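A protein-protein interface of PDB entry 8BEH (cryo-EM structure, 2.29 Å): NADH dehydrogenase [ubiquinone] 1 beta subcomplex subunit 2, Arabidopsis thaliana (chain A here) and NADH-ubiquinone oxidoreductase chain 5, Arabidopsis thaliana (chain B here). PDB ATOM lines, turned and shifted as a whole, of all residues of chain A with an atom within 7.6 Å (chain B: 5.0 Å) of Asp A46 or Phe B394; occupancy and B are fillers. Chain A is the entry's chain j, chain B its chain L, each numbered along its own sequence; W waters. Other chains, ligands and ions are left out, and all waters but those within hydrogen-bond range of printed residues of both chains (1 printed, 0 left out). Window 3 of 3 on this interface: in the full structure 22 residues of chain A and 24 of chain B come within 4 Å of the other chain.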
ATOM      1  N   MET A  35      16.262 -14.159 -12.152  1.00  0.00           N
ATOM      2  CA  MET A  35      17.352 -13.781 -11.256  1.00  0.00           C
ATOM      3  C   MET A  35      18.546 -14.724 -11.391  1.00  0.00           C
ATOM      4  O   MET A  35      19.697 -14.276 -11.458  1.00  0.00           O
ATOM      5  CB  MET A  35      16.847 -13.750  -9.814  1.00  0.00           C
ATOM      6  CG  MET A  35      17.938 -13.814  -8.759  1.00  0.00           C
ATOM      7  SD  MET A  35      17.289 -13.871  -7.077  1.00  0.00           S
ATOM      8  CE  MET A  35      16.536 -15.498  -7.059  1.00  0.00           C
ATOM      9  N   TRP A  38      20.262 -14.103 -14.701  1.00  0.00           N
ATOM     10  CA  TRP A  38      20.989 -12.843 -14.653  1.00  0.00           C
ATOM     11  C   TRP A  38      22.296 -12.996 -13.890  1.00  0.00           C
ATOM     12  O   TRP A  38      23.332 -12.467 -14.308  1.00  0.00           O
ATOM     13  CB  TRP A  38      20.101 -11.773 -14.021  1.00  0.00           C
ATOM     14  CG  TRP A  38      20.793 -10.508 -13.652  1.00  0.00           C
ATOM     15  CD1 TRP A  38      21.171 -10.123 -12.406  1.00  0.00           C
ATOM     16  CD2 TRP A  38      21.175  -9.451 -14.534  1.00  0.00           C
ATOM     17  NE1 TRP A  38      21.767  -8.888 -12.452  1.00  0.00           N
ATOM     18  CE2 TRP A  38      21.784  -8.454 -13.749  1.00  0.00           C
ATOM     19  CE3 TRP A  38      21.070  -9.254 -15.913  1.00  0.00           C
ATOM     20  CZ2 TRP A  38      22.281  -7.276 -14.297  1.00  0.00           C
ATOM     21  CZ3 TRP A  38      21.562  -8.081 -16.452  1.00  0.00           C
ATOM     22  CH2 TRP A  38      22.162  -7.110 -15.647  1.00  0.00           C
ATOM     23  N   ILE A  39      22.269 -13.732 -12.780  1.00  0.00           N
ATOM     24  CA  ILE A  39      23.493 -13.963 -12.021  1.00  0.00           C
ATOM     25  C   ILE A  39      24.505 -14.738 -12.858  1.00  0.00           C
ATOM     26  O   ILE A  39      25.692 -14.404 -12.883  1.00  0.00           O
ATOM     27  CB  ILE A  39      23.176 -14.681 -10.698  1.00  0.00           C
ATOM     28  CG1 ILE A  39      22.451 -13.733  -9.741  1.00  0.00           C
ATOM     29  CG2 ILE A  39      24.450 -15.222 -10.054  1.00  0.00           C
ATOM     30  CD1 ILE A  39      21.848 -14.423  -8.547  1.00  0.00           C
ATOM     31  N   LEU A  40      24.052 -15.783 -13.558  1.00  0.00           N
ATOM     32  CA  LEU A  40      24.972 -16.577 -14.371  1.00  0.00           C
ATOM     33  C   LEU A  40      25.577 -15.749 -15.500  1.00  0.00           C
ATOM     34  O   LEU A  40      26.791 -15.797 -15.742  1.00  0.00           O
ATOM     35  CB  LEU A  40      24.249 -17.799 -14.930  1.00  0.00           C
ATOM     36  CG  LEU A  40      23.878 -18.863 -13.900  1.00  0.00           C
ATOM     37  CD1 LEU A  40      23.103 -19.991 -14.550  1.00  0.00           C
ATOM     38  CD2 LEU A  40      25.115 -19.390 -13.188  1.00  0.00           C
ATOM     39  N   TYR A  41      24.743 -14.973 -16.192  1.00  0.00           N
ATOM     40  CA  TYR A  41      25.213 -14.143 -17.294  1.00  0.00           C
ATOM     41  C   TYR A  41      26.206 -13.097 -16.807  1.00  0.00           C
ATOM     42  O   TYR A  41      27.269 -12.905 -17.412  1.00  0.00           O
ATOM     43  CB  TYR A  41      24.011 -13.492 -17.980  1.00  0.00           C
ATOM     44  CG  TYR A  41      24.336 -12.628 -19.177  1.00  0.00           C
ATOM     45  CD1 TYR A  41      24.695 -11.295 -19.019  1.00  0.00           C
ATOM     46  CD2 TYR A  41      24.270 -13.140 -20.466  1.00  0.00           C
ATOM     47  CE1 TYR A  41      24.981 -10.501 -20.100  1.00  0.00           C
ATOM     48  CE2 TYR A  41      24.561 -12.351 -21.555  1.00  0.00           C
ATOM     49  CZ  TYR A  41      24.915 -11.031 -21.366  1.00  0.00           C
ATOM     50  OH  TYR A  41      25.208 -10.237 -22.444  1.00  0.00           O
ATOM     51  N   ARG A  42      25.884 -12.422 -15.698  1.00  0.00           N
ATOM     52  CA  ARG A  42      26.787 -11.415 -15.155  1.00  0.00           C
ATOM     53  C   ARG A  42      28.093 -12.041 -14.699  1.00  0.00           C
ATOM     54  O   ARG A  42      29.165 -11.453 -14.878  1.00  0.00           O
ATOM     55  CB  ARG A  42      26.120 -10.679 -13.995  1.00  0.00           C
ATOM     56  CG  ARG A  42      25.151  -9.597 -14.413  1.00  0.00           C
ATOM     57  CD  ARG A  42      25.785  -8.226 -14.339  1.00  0.00           C
ATOM     58  NE  ARG A  42      26.712  -7.985 -15.439  1.00  0.00           N
ATOM     59  CZ  ARG A  42      26.349  -7.776 -16.697  1.00  0.00           C
ATOM     60  NH1 ARG A  42      25.079  -7.791 -17.062  1.00  0.00           N
ATOM     61  NH2 ARG A  42      27.284  -7.540 -17.610  1.00  0.00           N
ATOM     62  N   ALA A  43      28.024 -13.223 -14.086  1.00  0.00           N
ATOM     63  CA  ALA A  43      29.239 -13.902 -13.662  1.00  0.00           C
ATOM     64  C   ALA A  43      30.129 -14.196 -14.858  1.00  0.00           C
ATOM     65  O   ALA A  43      31.312 -13.858 -14.854  1.00  0.00           O
ATOM     66  CB  ALA A  43      28.892 -15.183 -12.904  1.00  0.00           C
ATOM     67  N   LYS A  44      29.553 -14.747 -15.925  1.00  0.00           N
ATOM     68  CA  LYS A  44      30.353 -15.016 -17.115  1.00  0.00           C
ATOM     69  C   LYS A  44      30.942 -13.735 -17.702  1.00  0.00           C
ATOM     70  O   LYS A  44      32.111 -13.712 -18.102  1.00  0.00           O
ATOM     71  CB  LYS A  44      29.514 -15.754 -18.155  1.00  0.00           C
ATOM     72  CG  LYS A  44      29.892 -15.451 -19.582  1.00  0.00           C
ATOM     73  CD  LYS A  44      29.892 -16.708 -20.420  1.00  0.00           C
ATOM     74  CE  LYS A  44      29.799 -16.369 -21.889  1.00  0.00           C
ATOM     75  NZ  LYS A  44      28.571 -15.573 -22.153  1.00  0.00           N
ATOM     76  N   GLN A  45      30.159 -12.653 -17.749  1.00  0.00           N
ATOM     77  CA  GLN A  45      30.636 -11.434 -18.398  1.00  0.00           C
ATOM     78  C   GLN A  45      31.739 -10.757 -17.593  1.00  0.00           C
ATOM     79  O   GLN A  45      32.774 -10.373 -18.148  1.00  0.00           O
ATOM     80  CB  GLN A  45      29.484 -10.459 -18.634  1.00  0.00           C
ATOM     81  CG  GLN A  45      28.631 -10.785 -19.839  1.00  0.00           C
ATOM     82  CD  GLN A  45      29.286 -10.367 -21.136  1.00  0.00           C
ATOM     83  OE1 GLN A  45      29.564 -11.201 -21.998  1.00  0.00           O
ATOM     84  NE2 GLN A  45      29.546  -9.073 -21.281  1.00  0.00           N
ATOM     85  N   ASP A  46      31.544 -10.591 -16.288  1.00  0.00           N
ATOM     86  CA  ASP A  46      32.478  -9.796 -15.500  1.00  0.00           C
ATOM     87  C   ASP A  46      32.813 -10.473 -14.178  1.00  0.00           C
ATOM     88  O   ASP A  46      32.820  -9.836 -13.122  1.00  0.00           O
ATOM     89  CB  ASP A  46      31.933  -8.385 -15.264  1.00  0.00           C
ATOM     90  CG  ASP A  46      30.491  -8.381 -14.827  1.00  0.00           C
ATOM     91  OD1 ASP A  46      30.198  -8.925 -13.744  1.00  0.00           O
ATOM     92  OD2 ASP A  46      29.646  -7.839 -15.567  1.00  0.00           O
ATOM     93  N   GLY A  47      33.117 -11.764 -14.215  1.00  0.00           N
ATOM     94  CA  GLY A  47      33.588 -12.469 -13.050  1.00  0.00           C
ATOM     95  C   GLY A  47      35.091 -12.652 -12.993  1.00  0.00           C
ATOM     96  O   GLY A  47      35.682 -12.634 -11.911  1.00  0.00           O
ATOM     97  N   PRO A  48      35.734 -12.830 -14.195  1.00  0.00           N
ATOM     98  CA  PRO A  48      37.178 -12.866 -14.223  1.00  0.00           C
ATOM     99  C   PRO A  48      37.656 -11.491 -13.763  1.00  0.00           C
ATOM    100  O   PRO A  48      38.676 -11.450 -13.154  1.00  0.00           O
ATOM    101  CB  PRO A  48      37.517 -13.253 -15.653  1.00  0.00           C
ATOM    102  CG  PRO A  48      36.317 -14.001 -16.110  1.00  0.00           C
ATOM    103  CD  PRO A  48      35.211 -13.157 -15.542  1.00  0.00           C
ATOM    104  N   VAL A  49      36.901 -10.426 -14.015  1.00  0.00           N
ATOM    105  CA  VAL A  49      37.467  -9.107 -13.570  1.00  0.00           C
ATOM    106  C   VAL A  49      37.466  -8.994 -12.040  1.00  0.00           C
ATOM    107  O   VAL A  49      38.494  -8.629 -11.508  1.00  0.00           O
ATOM    108  CB  VAL A  49      36.858  -7.907 -14.305  1.00  0.00           C
ATOM    109  CG1 VAL A  49      37.131  -6.591 -13.601  1.00  0.00           C
ATOM    110  CG2 VAL A  49      37.301  -7.848 -15.753  1.00  0.00           C
ATOM    111  N   VAL A  50      36.375  -9.376 -11.366  1.00  0.00           N
ATOM    112  CA  VAL A  50      36.264  -9.328  -9.909  1.00  0.00           C
ATOM    113  C   VAL A  50      37.206 -10.341  -9.270  1.00  0.00           C
ATOM    114  O   VAL A  50      37.732 -10.115  -8.175  1.00  0.00           O
ATOM    115  CB  VAL A  50      34.801  -9.532  -9.461  1.00  0.00           C
ATOM    116  CG1 VAL A  50      33.860  -8.726 -10.336  1.00  0.00           C
ATOM    117  CG2 VAL A  50      34.410 -10.996  -9.484  1.00  0.00           C
ATOM    118  N   MET A  51      37.346 -11.532  -9.888  1.00  0.00           N
ATOM    119  CA  MET A  51      38.342 -12.515  -9.393  1.00  0.00           C
ATOM    120  C   MET A  51      39.741 -11.928  -9.526  1.00  0.00           C
ATOM    121  O   MET A  51      40.638 -12.434  -8.851  1.00  0.00           O
ATOM    122  CB  MET A  51      38.321 -13.834 -10.183  1.00  0.00           C
ATOM    123  CG  MET A  51      38.255 -15.038  -9.289  1.00  0.00           C
ATOM    124  SD  MET A  51      37.176 -14.686  -7.889  1.00  0.00           S
ATOM    125  CE  MET A  51      35.591 -14.685  -8.730  1.00  0.00           C
ATOM    126  N   ARG A  54      41.865 -11.018 -14.968  1.00  0.00           N
ATOM    127  CA  ARG A  54      42.175 -10.008 -15.994  1.00  0.00           C
ATOM    128  C   ARG A  54      41.660  -8.593 -15.684  1.00  0.00           C
ATOM    129  O   ARG A  54      41.007  -8.398 -14.687  1.00  0.00           O
ATOM    130  CB  ARG A  54      41.511 -10.394 -17.304  1.00  0.00           C
ATOM    131  CG  ARG A  54      40.016 -10.641 -17.170  1.00  0.00           C
ATOM    132  CD  ARG A  54      39.377 -10.996 -18.484  1.00  0.00           C
ATOM    133  NE  ARG A  54      39.616  -9.932 -19.435  1.00  0.00           N
ATOM    134  CZ  ARG A  54      38.810  -8.897 -19.620  1.00  0.00           C
ATOM    135  NH1 ARG A  54      37.703  -8.786 -18.909  1.00  0.00           N
ATOM    136  NH2 ARG A  54      39.122  -7.969 -20.503  1.00  0.00           N
ATOM    137  N   PHE B 392      24.527 -10.419  -2.479  1.00  0.00           N
ATOM    138  CA  PHE B 392      24.783 -11.505  -3.412  1.00  0.00           C
ATOM    139  C   PHE B 392      25.306 -10.938  -4.730  1.00  0.00           C
ATOM    140  O   PHE B 392      24.772  -9.942  -5.229  1.00  0.00           O
ATOM    141  CB  PHE B 392      23.515 -12.324  -3.659  1.00  0.00           C
ATOM    142  CG  PHE B 392      23.781 -13.714  -4.178  1.00  0.00           C
ATOM    143  CD1 PHE B 392      23.946 -13.940  -5.533  1.00  0.00           C
ATOM    144  CD2 PHE B 392      23.879 -14.788  -3.310  1.00  0.00           C
ATOM    145  CE1 PHE B 392      24.200 -15.215  -6.018  1.00  0.00           C
ATOM    146  CE2 PHE B 392      24.126 -16.062  -3.784  1.00  0.00           C
ATOM    147  CZ  PHE B 392      24.287 -16.277  -5.142  1.00  0.00           C
ATOM    148  N   PRO B 393      26.337 -11.546  -5.313  1.00  0.00           N
ATOM    149  CA  PRO B 393      27.001 -10.947  -6.478  1.00  0.00           C
ATOM    150  C   PRO B 393      26.043 -10.586  -7.603  1.00  0.00           C
ATOM    151  O   PRO B 393      25.153 -11.358  -7.965  1.00  0.00           O
ATOM    152  CB  PRO B 393      27.988 -12.036  -6.907  1.00  0.00           C
ATOM    153  CG  PRO B 393      28.332 -12.729  -5.634  1.00  0.00           C
ATOM    154  CD  PRO B 393      27.089 -12.693  -4.776  1.00  0.00           C
ATOM    155  N   PHE B 394      26.231  -9.381  -8.139  1.00  0.00           N
ATOM    156  CA  PHE B 394      25.569  -8.815  -9.311  1.00  0.00           C
ATOM    157  C   PHE B 394      24.104  -8.466  -9.077  1.00  0.00           C
ATOM    158  O   PHE B 394      23.439  -8.009 -10.007  1.00  0.00           O
ATOM    159  CB  PHE B 394      25.709  -9.733 -10.534  1.00  0.00           C
ATOM    160  CG  PHE B 394      27.076 -10.332 -10.662  1.00  0.00           C
ATOM    161  CD1 PHE B 394      28.172  -9.526 -10.920  1.00  0.00           C
ATOM    162  CD2 PHE B 394      27.276 -11.690 -10.490  1.00  0.00           C
ATOM    163  CE1 PHE B 394      29.437 -10.067 -11.015  1.00  0.00           C
ATOM    164  CE2 PHE B 394      28.535 -12.232 -10.591  1.00  0.00           C
ATOM    165  CZ  PHE B 394      29.617 -11.419 -10.856  1.00  0.00           C
ATOM    166  N   LEU B 395      23.585  -8.646  -7.871  1.00  0.00           N
ATOM    167  CA  LEU B 395      22.286  -8.108  -7.507  1.00  0.00           C
ATOM    168  C   LEU B 395      22.456  -6.656  -7.062  1.00  0.00           C
ATOM    169  O   LEU B 395      23.571  -6.159  -6.907  1.00  0.00           O
ATOM    170  CB  LEU B 395      21.649  -8.964  -6.414  1.00  0.00           C
ATOM    171  CG  LEU B 395      21.156 -10.353  -6.832  1.00  0.00           C
ATOM    172  CD1 LEU B 395      20.060 -10.841  -5.901  1.00  0.00           C
ATOM    173  CD2 LEU B 395      20.670 -10.346  -8.274  1.00  0.00           C
ATOM    174  N   THR B 396      21.331  -5.974  -6.843  1.00  0.00           N
ATOM    175  CA  THR B 396      21.372  -4.524  -6.657  1.00  0.00           C
ATOM    176  C   THR B 396      22.226  -4.127  -5.457  1.00  0.00           C
ATOM    177  O   THR B 396      23.041  -3.204  -5.550  1.00  0.00           O
ATOM    178  CB  THR B 396      19.954  -3.970  -6.522  1.00  0.00           C
ATOM    179  OG1 THR B 396      19.329  -3.956  -7.808  1.00  0.00           O
ATOM    180  CG2 THR B 396      19.967  -2.561  -5.962  1.00  0.00           C
ATOM    181  N   PHE B 398      24.735  -5.636  -4.210  1.00  0.00           N
ATOM    182  CA  PHE B 398      26.143  -5.980  -4.397  1.00  0.00           C
ATOM    183  C   PHE B 398      26.970  -4.791  -4.874  1.00  0.00           C
ATOM    184  O   PHE B 398      28.148  -4.679  -4.525  1.00  0.00           O
ATOM    185  CB  PHE B 398      26.244  -7.148  -5.383  1.00  0.00           C
ATOM    186  CG  PHE B 398      27.637  -7.419  -5.897  1.00  0.00           C
ATOM    187  CD1 PHE B 398      28.085  -6.841  -7.076  1.00  0.00           C
ATOM    188  CD2 PHE B 398      28.488  -8.266  -5.213  1.00  0.00           C
ATOM    189  CE1 PHE B 398      29.359  -7.104  -7.552  1.00  0.00           C
ATOM    190  CE2 PHE B 398      29.757  -8.529  -5.683  1.00  0.00           C
ATOM    191  CZ  PHE B 398      30.194  -7.951  -6.854  1.00  0.00           C
ATOM    192  N   TYR B 399      26.453  -3.952  -5.726  1.00  0.00           N
ATOM    193  CA  TYR B 399      27.236  -2.859  -6.330  1.00  0.00           C
ATOM    194  C   TYR B 399      27.563  -1.681  -5.375  1.00  0.00           C
ATOM    195  O   TYR B 399      28.449  -0.926  -5.698  1.00  0.00           O
ATOM    196  CB  TYR B 399      26.499  -2.374  -7.576  1.00  0.00           C
ATOM    197  CG  TYR B 399      26.453  -3.386  -8.682  1.00  0.00           C
ATOM    198  CD1 TYR B 399      27.551  -3.573  -9.506  1.00  0.00           C
ATOM    199  CD2 TYR B 399      25.342  -4.187  -8.873  1.00  0.00           C
ATOM    200  CE1 TYR B 399      27.537  -4.518 -10.512  1.00  0.00           C
ATOM    201  CE2 TYR B 399      25.315  -5.136  -9.876  1.00  0.00           C
ATOM    202  CZ  TYR B 399      26.411  -5.288 -10.706  1.00  0.00           C
ATOM    203  OH  TYR B 399      26.406  -6.218 -11.693  1.00  0.00           O
ATOM    204  N   LEU B 475      16.680  -6.480  -8.539  1.00  0.00           N
ATOM    205  CA  LEU B 475      17.556  -7.244  -9.418  1.00  0.00           C
ATOM    206  C   LEU B 475      18.436  -6.367 -10.296  1.00  0.00           C
ATOM    207  O   LEU B 475      19.619  -6.671 -10.463  1.00  0.00           O
ATOM    208  CB  LEU B 475      16.751  -8.189 -10.315  1.00  0.00           C
ATOM    209  CG  LEU B 475      15.973  -9.305  -9.622  1.00  0.00           C
ATOM    210  CD1 LEU B 475      15.065 -10.010 -10.614  1.00  0.00           C
ATOM    211  CD2 LEU B 475      16.910 -10.275  -8.935  1.00  0.00           C
HETATM  212  O   HOH W   1      28.930  -6.342 -12.780  1.00  0.00           O
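The indole nitrogen of Trp A38 lies within hydrogen-bond range of the backbone carbonyl oxygen of Phe B394 (3.1 Å).
Printed residues of chain B that touch a printed residue of chain A: Phe B392, Phe B394, Tyr B399 and Leu B475. Hydrophobic or aromatic side chains of chain B within 4 Å of the printed part of chain A: Phe B392, Phe B394, Tyr B399 and Leu B475. Along chain B the printed residues that touch a printed residue of chain A span positions 392 to 475. Of the 16 printed residues of chain A, 6 touch a printed residue of chain B. Hydrophobic or aromatic side chains of chain A that line the printed part of chain B: Met A35, Trp A38, Ile A39 and Ala A43. Among the printed residues, 9 pairs touch across the chains.
NE of Arg A42 is in salt-bridge range of OD2 of Asp A46.
Among the printed residues, merely in contact across the chains: Asp A46 with Phe B394 (3.1 Å), Arg A42 with Tyr B399 (3.4 Å), Arg A42 with Phe B394 (3.5 Å), Ile A39 with Phe B392 (3.5 Å), Ala A43 with Phe B394 (3.6 Å), Met A35 with Leu B475 (3.6 Å), Trp A38 with Leu B475 (3.7 Å) and Ile A39 with Phe B394 (3.9 Å).
Water W1 bridges OH of Tyr B399 and OD1 of Asp A46.
Of the printed residues of chain B, Asp A46 touches Phe B394. Phe B394 touches just these residues of chain A: Trp A38, Ile A39, Arg A42, Ala A43 and Asp A46. Printed residues of chain B within 4 Å of Arg A42: Phe B394 (3.5 Å) and Tyr B399 (3.4 Å). Of the printed residues of chain A, Leu B475 touches Met A35 and Trp A38. Printed residues of chain B within 4 Å of Ala A43: Phe B394. Printed residues of chain B within 4 Å of Met A35: Leu B475. Printed residues of chain B within 4 Å of Ile A39: Phe B392 and Phe B394. The nearest printed residue of chain B that does not touch Asp A46 is Tyr B399 (5.1 Å).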
